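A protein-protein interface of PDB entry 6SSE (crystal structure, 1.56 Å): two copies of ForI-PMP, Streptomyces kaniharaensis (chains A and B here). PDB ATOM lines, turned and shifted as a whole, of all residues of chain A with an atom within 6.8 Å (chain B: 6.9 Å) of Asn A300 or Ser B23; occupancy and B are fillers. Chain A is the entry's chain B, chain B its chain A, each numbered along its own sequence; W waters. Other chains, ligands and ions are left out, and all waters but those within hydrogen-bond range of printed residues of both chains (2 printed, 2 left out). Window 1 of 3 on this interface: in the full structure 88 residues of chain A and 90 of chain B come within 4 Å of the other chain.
OD1 of Asn B22 is in hydrogen-bond range of N of Thr B25, 3.5 Å away.
The guanidinium group (NH2) of Arg B24 lies within hydrogen-bond range of the side-chain amide oxygen (OD1) of Asn B58 (2.7 Å).
ND2 of Asn A300 lies close to NE2 of His A295 (3.3 Å).
O of Gly A297 lies close to OD1 of Asn A300.
ND2 of Asn B22 is in hydrogen-bond range of O of Arg B24 (2.9 Å).
The backbone carbonyl oxygen (O) of Ser A296 sits at hydrogen-bond distance from the side-chain amide nitrogen (ND2) of Asn A300 (3.0 Å).
Asn A300 touches just these residues of chain B: Ser B23 (3.2 Å) and Arg B24 (3.97 Å).
Printed residues of chain A within 4 Å of Ser B23: Arg A110 (3.5 Å), Phe A111 (2.8 Å) and Asn A300 (3.2 Å).
Of the printed residues of chain B, Phe A85 touches Arg B24 (2.9 Å) and Asn B58 (3.1 Å).
Of the printed residues of chain B, Val A109 touches Met B18 (3.5 Å) and Pro B19 (3.4 Å).
Printed residues of chain B within 4 Å of Ser A298: Arg B24 and Asn B58.
The nearest residue of chain B that does not touch Asn A300 is Thr B25 (5.7 Å).
The nearest printed residue of chain A that does not touch Pro B19 is Phe A111 (7.3 Å).
Printed residues of chain A that touch a printed residue of chain B: Phe A85, Glu A92, Val A109, Arg A110, Phe A111, Pro A286, His A295, Ser A296, Gly A297, Ser A298 and Asn A300.
Hydrophobic or aromatic side chains of chain A within 4 Å of the printed part of chain B: Phe A111 and Pro A286.
Printed residues of chain B that touch a printed residue of chain A: Met B18, Pro B19, Asn B22, Ser B23, Arg B24, Thr B25, Ala B26 and Asn B58.
Among the printed residues, 23 pairs touch across the chains.
CG of Met B18 touches O of Val A109 (3.5 Å).
O of Val A109 touches CD of Pro B19, 3.4 Å away.
Pro B19 touches Arg A110 (CD to CG, 3.7 Å).
Ser B23 touches Arg A110 (C to NH2, 3.5 Å).
Met B18 touches Phe A111 (CE to CE2, 3.98 Å).
CD of Pro A286 touches O of Pro B19, 3.7 Å away.
Asn B22 touches Pro A286.
Arg B24 touches His A295.
Arg B24 touches Ser A298 (NH1 to O, 3.6 Å).
Asn A300 touches Arg B24.
No position is printed for both chains.
Water W2 lies within hydrogen-bond range of OE2 of Glu A92 and N of Ser B23.
Water W1 bridges O of Asn A300 and NH1 of Arg B24.
OG of Ser B23 is in hydrogen-bond range of N of Phe A111 (2.8 Å).
NH1 of Arg B24 lies within hydrogen-bond range of O of Phe A85 (2.9 Å).
The side-chain sulfur (SD) of Met B18 lies close to the side-chain carboxylate (OE2) of Glu A92.
OG1 of Thr B25 sits at hydrogen-bond distance from NH2 of Arg A110 (3.4 Å).
The guanidinium group of Arg A110 lies close to the backbone NH of Arg B24.
OD1 of Asn B58 sits close to O of Phe A85, 3.1 Å away.
N of Thr B25 is in hydrogen-bond range of OG of Ser A296 (3.4 Å).
The backbone NH of Ala B26 sits at hydrogen-bond distance from the side-chain hydroxyl of Ser A296, 3.0 Å away.
The backbone carbonyl oxygen (O) of Asn B22 sits at hydrogen-bond distance from the guanidinium group (NH1) of Arg A110.
The side-chain hydroxyl (OG1) of Thr B25 sits at hydrogen-bond distance from the backbone NH (N) of His A295 (2.8 Å).
O of Gly A297 is in hydrogen-bond range of NE of Arg B24, at 3.1 Å.
The backbone carbonyl oxygen (O) of Ser B23 is in hydrogen-bond range of the side-chain amide nitrogen (ND2) of Asn A300.
ND2 of Asn B58 lies within hydrogen-bond range of O of Ser A298 (3.0 Å).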
ATOM      1  N   PHE A  85     -17.866  17.813  32.975  1.00  0.00           N
ATOM      2  CA  PHE A  85     -18.165  16.545  32.263  1.00  0.00           C
ATOM      3  C   PHE A  85     -17.672  16.642  30.819  1.00  0.00           C
ATOM      4  O   PHE A  85     -17.642  17.722  30.243  1.00  0.00           O
ATOM      5  CB  PHE A  85     -19.678  16.339  32.205  1.00  0.00           C
ATOM      6  CG  PHE A  85     -20.338  16.167  33.551  1.00  0.00           C
ATOM      7  CD1 PHE A  85     -20.454  14.909  34.112  1.00  0.00           C
ATOM      8  CD2 PHE A  85     -20.890  17.228  34.239  1.00  0.00           C
ATOM      9  CE1 PHE A  85     -21.111  14.736  35.319  1.00  0.00           C
ATOM     10  CE2 PHE A  85     -21.473  17.057  35.486  1.00  0.00           C
ATOM     11  CZ  PHE A  85     -21.550  15.812  36.042  1.00  0.00           C
ATOM     12  N   GLU A  92     -26.470  23.981  30.478  1.00  0.00           N
ATOM     13  CA  GLU A  92     -25.883  24.774  29.363  1.00  0.00           C
ATOM     14  C   GLU A  92     -27.015  25.283  28.480  1.00  0.00           C
ATOM     15  O   GLU A  92     -26.946  26.403  27.991  1.00  0.00           O
ATOM     16  CB  GLU A  92     -24.801  24.061  28.569  1.00  0.00           C
ATOM     17  CG  GLU A  92     -25.235  23.026  27.556  1.00  0.00           C
ATOM     18  CD  GLU A  92     -24.090  22.422  26.770  1.00  0.00           C
ATOM     19  OE1 GLU A  92     -23.150  21.875  27.444  1.00  0.00           O
ATOM     20  OE2 GLU A  92     -24.146  22.449  25.523  1.00  0.00           O
ATOM     21  N   VAL A 109     -25.215  31.287  20.802  1.00  0.00           N
ATOM     22  CA  VAL A 109     -24.151  31.608  21.792  1.00  0.00           C
ATOM     23  C   VAL A 109     -23.228  30.413  21.917  1.00  0.00           C
ATOM     24  O   VAL A 109     -23.637  29.243  21.683  1.00  0.00           O
ATOM     25  CB  VAL A 109     -24.770  31.992  23.150  1.00  0.00           C
ATOM     26  CG1 VAL A 109     -25.878  33.024  23.015  1.00  0.00           C
ATOM     27  CG2 VAL A 109     -25.287  30.815  23.920  1.00  0.00           C
ATOM     28  N   ARG A 110     -21.961  30.677  22.180  1.00  0.00           N
ATOM     29  CA  ARG A 110     -20.992  29.643  22.619  1.00  0.00           C
ATOM     30  C   ARG A 110     -20.302  30.127  23.886  1.00  0.00           C
ATOM     31  O   ARG A 110     -19.984  31.329  23.961  1.00  0.00           O
ATOM     32  CB  ARG A 110     -19.977  29.328  21.541  1.00  0.00           C
ATOM     33  CG  ARG A 110     -20.530  28.457  20.421  1.00  0.00           C
ATOM     34  CD  ARG A 110     -19.398  28.070  19.512  1.00  0.00           C
ATOM     35  NE  ARG A 110     -18.538  26.943  19.902  1.00  0.00           N
ATOM     36  CZ  ARG A 110     -18.739  25.667  19.531  1.00  0.00           C
ATOM     37  NH1 ARG A 110     -19.864  25.347  18.941  1.00  0.00           N
ATOM     38  NH2 ARG A 110     -17.831  24.737  19.781  1.00  0.00           N
ATOM     39  N   PHE A 111     -20.000  29.215  24.774  1.00  0.00           N
ATOM     40  CA  PHE A 111     -19.353  29.513  26.064  1.00  0.00           C
ATOM     41  C   PHE A 111     -17.870  29.145  26.035  1.00  0.00           C
ATOM     42  O   PHE A 111     -17.490  28.130  25.456  1.00  0.00           O
ATOM     43  CB  PHE A 111     -20.077  28.828  27.219  1.00  0.00           C
ATOM     44  CG  PHE A 111     -21.535  29.248  27.265  1.00  0.00           C
ATOM     45  CD1 PHE A 111     -21.869  30.572  27.527  1.00  0.00           C
ATOM     46  CD2 PHE A 111     -22.533  28.318  27.137  1.00  0.00           C
ATOM     47  CE1 PHE A 111     -23.201  30.965  27.573  1.00  0.00           C
ATOM     48  CE2 PHE A 111     -23.862  28.730  27.136  1.00  0.00           C
ATOM     49  CZ  PHE A 111     -24.187  30.025  27.430  1.00  0.00           C
ATOM     50  N   THR A 112     -17.097  30.013  26.677  1.00  0.00           N
ATOM     51  CA  THR A 112     -15.641  29.815  26.916  1.00  0.00           C
ATOM     52  C   THR A 112     -15.385  29.927  28.434  1.00  0.00           C
ATOM     53  O   THR A 112     -16.315  30.161  29.248  1.00  0.00           O
ATOM     54  CB  THR A 112     -14.851  30.876  26.152  1.00  0.00           C
ATOM     55  OG1 THR A 112     -15.157  32.108  26.825  1.00  0.00           O
ATOM     56  CG2 THR A 112     -15.145  30.979  24.680  1.00  0.00           C
ATOM     57  N   SER A 113     -14.116  29.778  28.866  1.00  0.00           N
ATOM     58  CA  SER A 113     -13.804  29.894  30.315  1.00  0.00           C
ATOM     59  C   SER A 113     -13.338  31.297  30.701  1.00  0.00           C
ATOM     60  O   SER A 113     -13.019  31.521  31.878  1.00  0.00           O
ATOM     61  CB  SER A 113     -12.802  28.895  30.755  1.00  0.00           C
ATOM     62  OG  SER A 113     -13.431  27.620  30.703  1.00  0.00           O
ATOM     63  N   GLU A 117     -10.532  34.336  26.147  1.00  0.00           N
ATOM     64  CA  GLU A 117     -10.809  33.266  25.177  1.00  0.00           C
ATOM     65  C   GLU A 117     -11.976  33.676  24.251  1.00  0.00           C
ATOM     66  O   GLU A 117     -11.966  33.308  23.072  1.00  0.00           O
ATOM     67  CB  GLU A 117     -11.222  31.957  25.877  1.00  0.00           C
ATOM     68  CG  GLU A 117     -10.082  31.176  26.500  1.00  0.00           C
ATOM     69  CD  GLU A 117     -10.528  29.778  26.975  1.00  0.00           C
ATOM     70  OE1 GLU A 117     -11.799  29.500  27.168  1.00  0.00           O
ATOM     71  OE2 GLU A 117      -9.637  28.944  27.265  1.00  0.00           O
ATOM     72  N   PRO A 286     -20.933  22.088  14.148  1.00  0.00           N
ATOM     73  CA  PRO A 286     -20.366  20.795  13.786  1.00  0.00           C
ATOM     74  C   PRO A 286     -21.371  19.755  13.252  1.00  0.00           C
ATOM     75  O   PRO A 286     -21.009  18.611  13.083  1.00  0.00           O
ATOM     76  CB  PRO A 286     -19.824  20.352  15.160  1.00  0.00           C
ATOM     77  CG  PRO A 286     -20.904  20.796  16.134  1.00  0.00           C
ATOM     78  CD  PRO A 286     -21.411  22.111  15.535  1.00  0.00           C
ATOM     79  N   HIS A 295     -13.825  24.494  18.086  1.00  0.00           N
ATOM     80  CA  HIS A 295     -13.763  25.286  19.343  1.00  0.00           C
ATOM     81  C   HIS A 295     -14.126  24.352  20.494  1.00  0.00           C
ATOM     82  O   HIS A 295     -15.277  24.190  20.764  1.00  0.00           O
ATOM     83  CB  HIS A 295     -14.651  26.512  19.284  1.00  0.00           C
ATOM     84  CG  HIS A 295     -14.757  27.155  20.616  1.00  0.00           C
ATOM     85  ND1 HIS A 295     -15.944  27.431  21.175  1.00  0.00           N
ATOM     86  CD2 HIS A 295     -13.789  27.465  21.516  1.00  0.00           C
ATOM     87  CE1 HIS A 295     -15.745  27.906  22.409  1.00  0.00           C
ATOM     88  NE2 HIS A 295     -14.407  27.943  22.635  1.00  0.00           N
ATOM     89  N   SER A 296     -13.101  23.861  21.176  1.00  0.00           N
ATOM     90  CA  SER A 296     -13.249  22.995  22.344  1.00  0.00           C
ATOM     91  C   SER A 296     -12.773  23.755  23.561  1.00  0.00           C
ATOM     92  O   SER A 296     -12.667  25.031  23.522  1.00  0.00           O
ATOM     93  CB  SER A 296     -12.646  21.699  22.075  1.00  0.00           C
ATOM     94  OG  SER A 296     -13.353  21.027  21.032  1.00  0.00           O
ATOM     95  N   GLY A 297     -12.494  23.037  24.641  1.00  0.00           N
ATOM     96  CA  GLY A 297     -12.083  23.646  25.917  1.00  0.00           C
ATOM     97  C   GLY A 297     -12.676  22.847  27.044  1.00  0.00           C
ATOM     98  O   GLY A 297     -13.910  22.684  27.093  1.00  0.00           O
ATOM     99  N   SER A 298     -11.837  22.370  27.956  1.00  0.00           N
ATOM    100  CA  SER A 298     -12.250  21.407  28.993  1.00  0.00           C
ATOM    101  C   SER A 298     -13.390  21.959  29.823  1.00  0.00           C
ATOM    102  O   SER A 298     -14.146  21.158  30.393  1.00  0.00           O
ATOM    103  CB  SER A 298     -11.049  21.035  29.868  1.00  0.00           C
ATOM    104  OG  SER A 298     -10.104  20.385  29.024  1.00  0.00           O
ATOM    105  N   TYR A 299     -13.436  23.261  30.068  1.00  0.00           N
ATOM    106  CA  TYR A 299     -14.423  23.845  30.997  1.00  0.00           C
ATOM    107  C   TYR A 299     -15.544  24.607  30.262  1.00  0.00           C
ATOM    108  O   TYR A 299     -16.394  25.205  30.915  1.00  0.00           O
ATOM    109  CB  TYR A 299     -13.753  24.689  32.065  1.00  0.00           C
ATOM    110  CG  TYR A 299     -12.488  24.043  32.576  1.00  0.00           C
ATOM    111  CD1 TYR A 299     -12.551  22.974  33.468  1.00  0.00           C
ATOM    112  CD2 TYR A 299     -11.265  24.387  32.073  1.00  0.00           C
ATOM    113  CE1 TYR A 299     -11.431  22.293  33.862  1.00  0.00           C
ATOM    114  CE2 TYR A 299     -10.112  23.721  32.472  1.00  0.00           C
ATOM    115  CZ  TYR A 299     -10.204  22.652  33.341  1.00  0.00           C
ATOM    116  OH  TYR A 299      -9.068  22.023  33.746  1.00  0.00           O
ATOM    117  N   ASN A 300     -15.593  24.537  28.930  1.00  0.00           N
ATOM    118  CA  ASN A 300     -16.641  25.217  28.165  1.00  0.00           C
ATOM    119  C   ASN A 300     -17.998  24.716  28.643  1.00  0.00           C
ATOM    120  O   ASN A 300     -18.221  23.450  28.655  1.00  0.00           O
ATOM    121  CB  ASN A 300     -16.561  24.921  26.669  1.00  0.00           C
ATOM    122  CG  ASN A 300     -15.374  25.537  25.926  1.00  0.00           C
ATOM    123  OD1 ASN A 300     -14.424  26.021  26.534  1.00  0.00           O
ATOM    124  ND2 ASN A 300     -15.453  25.448  24.595  1.00  0.00           N
ATOM    125  N   ALA A 301     -18.860  25.624  29.066  1.00  0.00           N
ATOM    126  CA  ALA A 301     -20.270  25.294  29.416  1.00  0.00           C
ATOM    127  C   ALA A 301     -20.284  24.360  30.628  1.00  0.00           C
ATOM    128  O   ALA A 301     -21.321  23.635  30.838  1.00  0.00           O
ATOM    129  CB  ALA A 301     -20.973  24.691  28.219  1.00  0.00           C
ATOM    130  N   ASN A 302     -19.248  24.384  31.481  1.00  0.00           N
ATOM    131  CA  ASN A 302     -19.253  23.521  32.677  1.00  0.00           C
ATOM    132  C   ASN A 302     -20.488  23.888  33.504  1.00  0.00           C
ATOM    133  O   ASN A 302     -20.842  25.070  33.657  1.00  0.00           O
ATOM    134  CB  ASN A 302     -17.921  23.561  33.420  1.00  0.00           C
ATOM    135  CG  ASN A 302     -17.809  24.807  34.272  1.00  0.00           C
ATOM    136  OD1 ASN A 302     -18.399  24.872  35.369  1.00  0.00           O
ATOM    137  ND2 ASN A 302     -17.108  25.828  33.750  1.00  0.00           N
ATOM    138  N   PRO A 303     -21.124  22.929  34.195  1.00  0.00           N
ATOM    139  CA  PRO A 303     -22.398  23.210  34.887  1.00  0.00           C
ATOM    140  C   PRO A 303     -22.263  24.124  36.099  1.00  0.00           C
ATOM    141  O   PRO A 303     -23.253  24.710  36.511  1.00  0.00           O
ATOM    142  CB  PRO A 303     -22.918  21.793  35.246  1.00  0.00           C
ATOM    143  CG  PRO A 303     -21.652  20.966  35.284  1.00  0.00           C
ATOM    144  CD  PRO A 303     -20.825  21.489  34.142  1.00  0.00           C
ATOM    145  N   MET A 306     -22.352  27.497  34.417  1.00  0.00           N
ATOM    146  CA  MET A 306     -23.712  27.678  33.846  1.00  0.00           C
ATOM    147  C   MET A 306     -24.681  27.984  34.991  1.00  0.00           C
ATOM    148  O   MET A 306     -25.551  28.833  34.783  1.00  0.00           O
ATOM    149  CB  MET A 306     -24.167  26.418  33.089  1.00  0.00           C
ATOM    150  CG  MET A 306     -23.271  26.042  31.889  1.00  0.00           C
ATOM    151  SD  MET A 306     -23.245  27.159  30.492  1.00  0.00           S
ATOM    152  CE  MET A 306     -21.933  28.294  30.995  1.00  0.00           C
ATOM    153  N   MET B  18     -27.641  27.744  20.188  1.00  0.00           N
ATOM    154  CA  MET B  18     -26.190  27.497  19.983  1.00  0.00           C
ATOM    155  C   MET B  18     -25.988  27.007  18.562  1.00  0.00           C
ATOM    156  O   MET B  18     -26.870  26.357  18.018  1.00  0.00           O
ATOM    157  CB  MET B  18     -25.666  26.392  20.902  1.00  0.00           C
ATOM    158  CG  MET B  18     -25.821  26.597  22.322  1.00  0.00           C
ATOM    159  SD  MET B  18     -25.152  25.099  23.150  1.00  0.00           S
ATOM    160  CE  MET B  18     -25.101  25.744  24.821  1.00  0.00           C
ATOM    161  N   PRO B  19     -24.807  27.242  17.952  1.00  0.00           N
ATOM    162  CA  PRO B  19     -24.552  26.782  16.595  1.00  0.00           C
ATOM    163  C   PRO B  19     -24.509  25.252  16.499  1.00  0.00           C
ATOM    164  O   PRO B  19     -23.634  24.596  17.104  1.00  0.00           O
ATOM    165  CB  PRO B  19     -23.191  27.372  16.219  1.00  0.00           C
ATOM    166  CG  PRO B  19     -22.674  28.079  17.430  1.00  0.00           C
ATOM    167  CD  PRO B  19     -23.668  27.933  18.555  1.00  0.00           C
ATOM    168  N   GLY B  20     -25.468  24.684  15.773  1.00  0.00           N
ATOM    169  CA  GLY B  20     -25.601  23.209  15.746  1.00  0.00           C
ATOM    170  C   GLY B  20     -25.845  22.643  17.141  1.00  0.00           C
ATOM    171  O   GLY B  20     -25.637  21.454  17.320  1.00  0.00           O
ATOM    172  N   GLY B  21     -26.375  23.431  18.076  1.00  0.00           N
ATOM    173  CA  GLY B  21     -26.695  22.975  19.442  1.00  0.00           C
ATOM    174  C   GLY B  21     -25.441  22.638  20.246  1.00  0.00           C
ATOM    175  O   GLY B  21     -25.511  21.812  21.157  1.00  0.00           O
ATOM    176  N   ASN B  22     -24.349  23.306  19.929  1.00  0.00           N
ATOM    177  CA  ASN B  22     -23.003  22.906  20.423  1.00  0.00           C
ATOM    178  C   ASN B  22     -22.247  24.097  21.002  1.00  0.00           C
ATOM    179  O   ASN B  22     -22.331  25.176  20.446  1.00  0.00           O
ATOM    180  CB  ASN B  22     -22.210  22.234  19.324  1.00  0.00           C
ATOM    181  CG  ASN B  22     -20.830  21.804  19.785  1.00  0.00           C
ATOM    182  OD1 ASN B  22     -19.838  22.385  19.344  1.00  0.00           O
ATOM    183  ND2 ASN B  22     -20.777  20.759  20.612  1.00  0.00           N
ATOM    184  N   SER B  23     -21.492  23.863  22.108  1.00  0.00           N
ATOM    185  CA  SER B  23     -20.645  24.900  22.735  1.00  0.00           C
ATOM    186  C   SER B  23     -19.216  24.379  22.947  1.00  0.00           C
ATOM    187  O   SER B  23     -18.406  25.108  23.523  1.00  0.00           O
ATOM    188  CB  SER B  23     -21.207  25.335  24.015  1.00  0.00           C
ATOM    189  OG  SER B  23     -20.483  26.448  24.542  1.00  0.00           O
ATOM    190  N   ARG B  24     -18.907  23.197  22.450  1.00  0.00           N
ATOM    191  CA  ARG B  24     -17.627  22.509  22.686  1.00  0.00           C
ATOM    192  C   ARG B  24     -17.517  21.400  21.633  1.00  0.00           C
ATOM    193  O   ARG B  24     -18.158  20.377  21.797  1.00  0.00           O
ATOM    194  CB  ARG B  24     -17.577  22.041  24.127  1.00  0.00           C
ATOM    195  CG  ARG B  24     -16.278  21.345  24.485  1.00  0.00           C
ATOM    196  CD  ARG B  24     -16.375  20.815  25.901  1.00  0.00           C
ATOM    197  NE  ARG B  24     -15.227  19.968  26.259  1.00  0.00           N
ATOM    198  CZ  ARG B  24     -15.201  19.208  27.355  1.00  0.00           C
ATOM    199  NH1 ARG B  24     -16.216  19.239  28.197  1.00  0.00           N
ATOM    200  NH2 ARG B  24     -14.112  18.517  27.613  1.00  0.00           N
ATOM    201  N   THR B  25     -16.699  21.567  20.644  1.00  0.00           N
ATOM    202  CA  THR B  25     -16.735  20.691  19.442  1.00  0.00           C
ATOM    203  C   THR B  25     -16.521  19.257  19.871  1.00  0.00           C
ATOM    204  O   THR B  25     -17.192  18.336  19.300  1.00  0.00           O
ATOM    205  CB  THR B  25     -15.720  21.157  18.401  1.00  0.00           C
ATOM    206  OG1 THR B  25     -15.857  22.564  18.123  1.00  0.00           O
ATOM    207  CG2 THR B  25     -15.873  20.362  17.116  1.00  0.00           C
ATOM    208  N   ALA B  26     -15.585  19.040  20.811  1.00  0.00           N
ATOM    209  CA  ALA B  26     -15.135  17.679  21.185  1.00  0.00           C
ATOM    210  C   ALA B  26     -16.271  16.856  21.788  1.00  0.00           C
ATOM    211  O   ALA B  26     -16.078  15.629  21.872  1.00  0.00           O
ATOM    212  CB  ALA B  26     -13.962  17.768  22.142  1.00  0.00           C
ATOM    213  N   VAL B  27     -17.335  17.448  22.300  1.00  0.00           N
ATOM    214  CA  VAL B  27     -18.395  16.662  22.981  1.00  0.00           C
ATOM    215  C   VAL B  27     -19.588  16.436  22.056  1.00  0.00           C
ATOM    216  O   VAL B  27     -20.519  15.731  22.493  1.00  0.00           O
ATOM    217  CB  VAL B  27     -18.808  17.300  24.307  1.00  0.00           C
ATOM    218  CG1 VAL B  27     -17.603  17.446  25.223  1.00  0.00           C
ATOM    219  CG2 VAL B  27     -19.632  18.564  24.107  1.00  0.00           C
ATOM    220  N   ASN B  58     -14.155  13.755  31.663  1.00  0.00           N
ATOM    221  CA  ASN B  58     -13.987  15.108  31.077  1.00  0.00           C
ATOM    222  C   ASN B  58     -12.614  15.249  30.426  1.00  0.00           C
ATOM    223  O   ASN B  58     -11.822  16.095  30.831  1.00  0.00           O
ATOM    224  CB  ASN B  58     -14.214  16.239  32.093  1.00  0.00           C
ATOM    225  CG  ASN B  58     -14.285  17.550  31.347  1.00  0.00           C
ATOM    226  OD1 ASN B  58     -14.527  17.512  30.138  1.00  0.00           O
ATOM    227  ND2 ASN B  58     -14.003  18.674  32.011  1.00  0.00           N
HETATM  228  O   HOH W   1     -18.833  20.811  27.886  1.00  0.00           O
HETATM  229  O   HOH W   2     -22.195  21.647  23.820  1.00  0.00           O
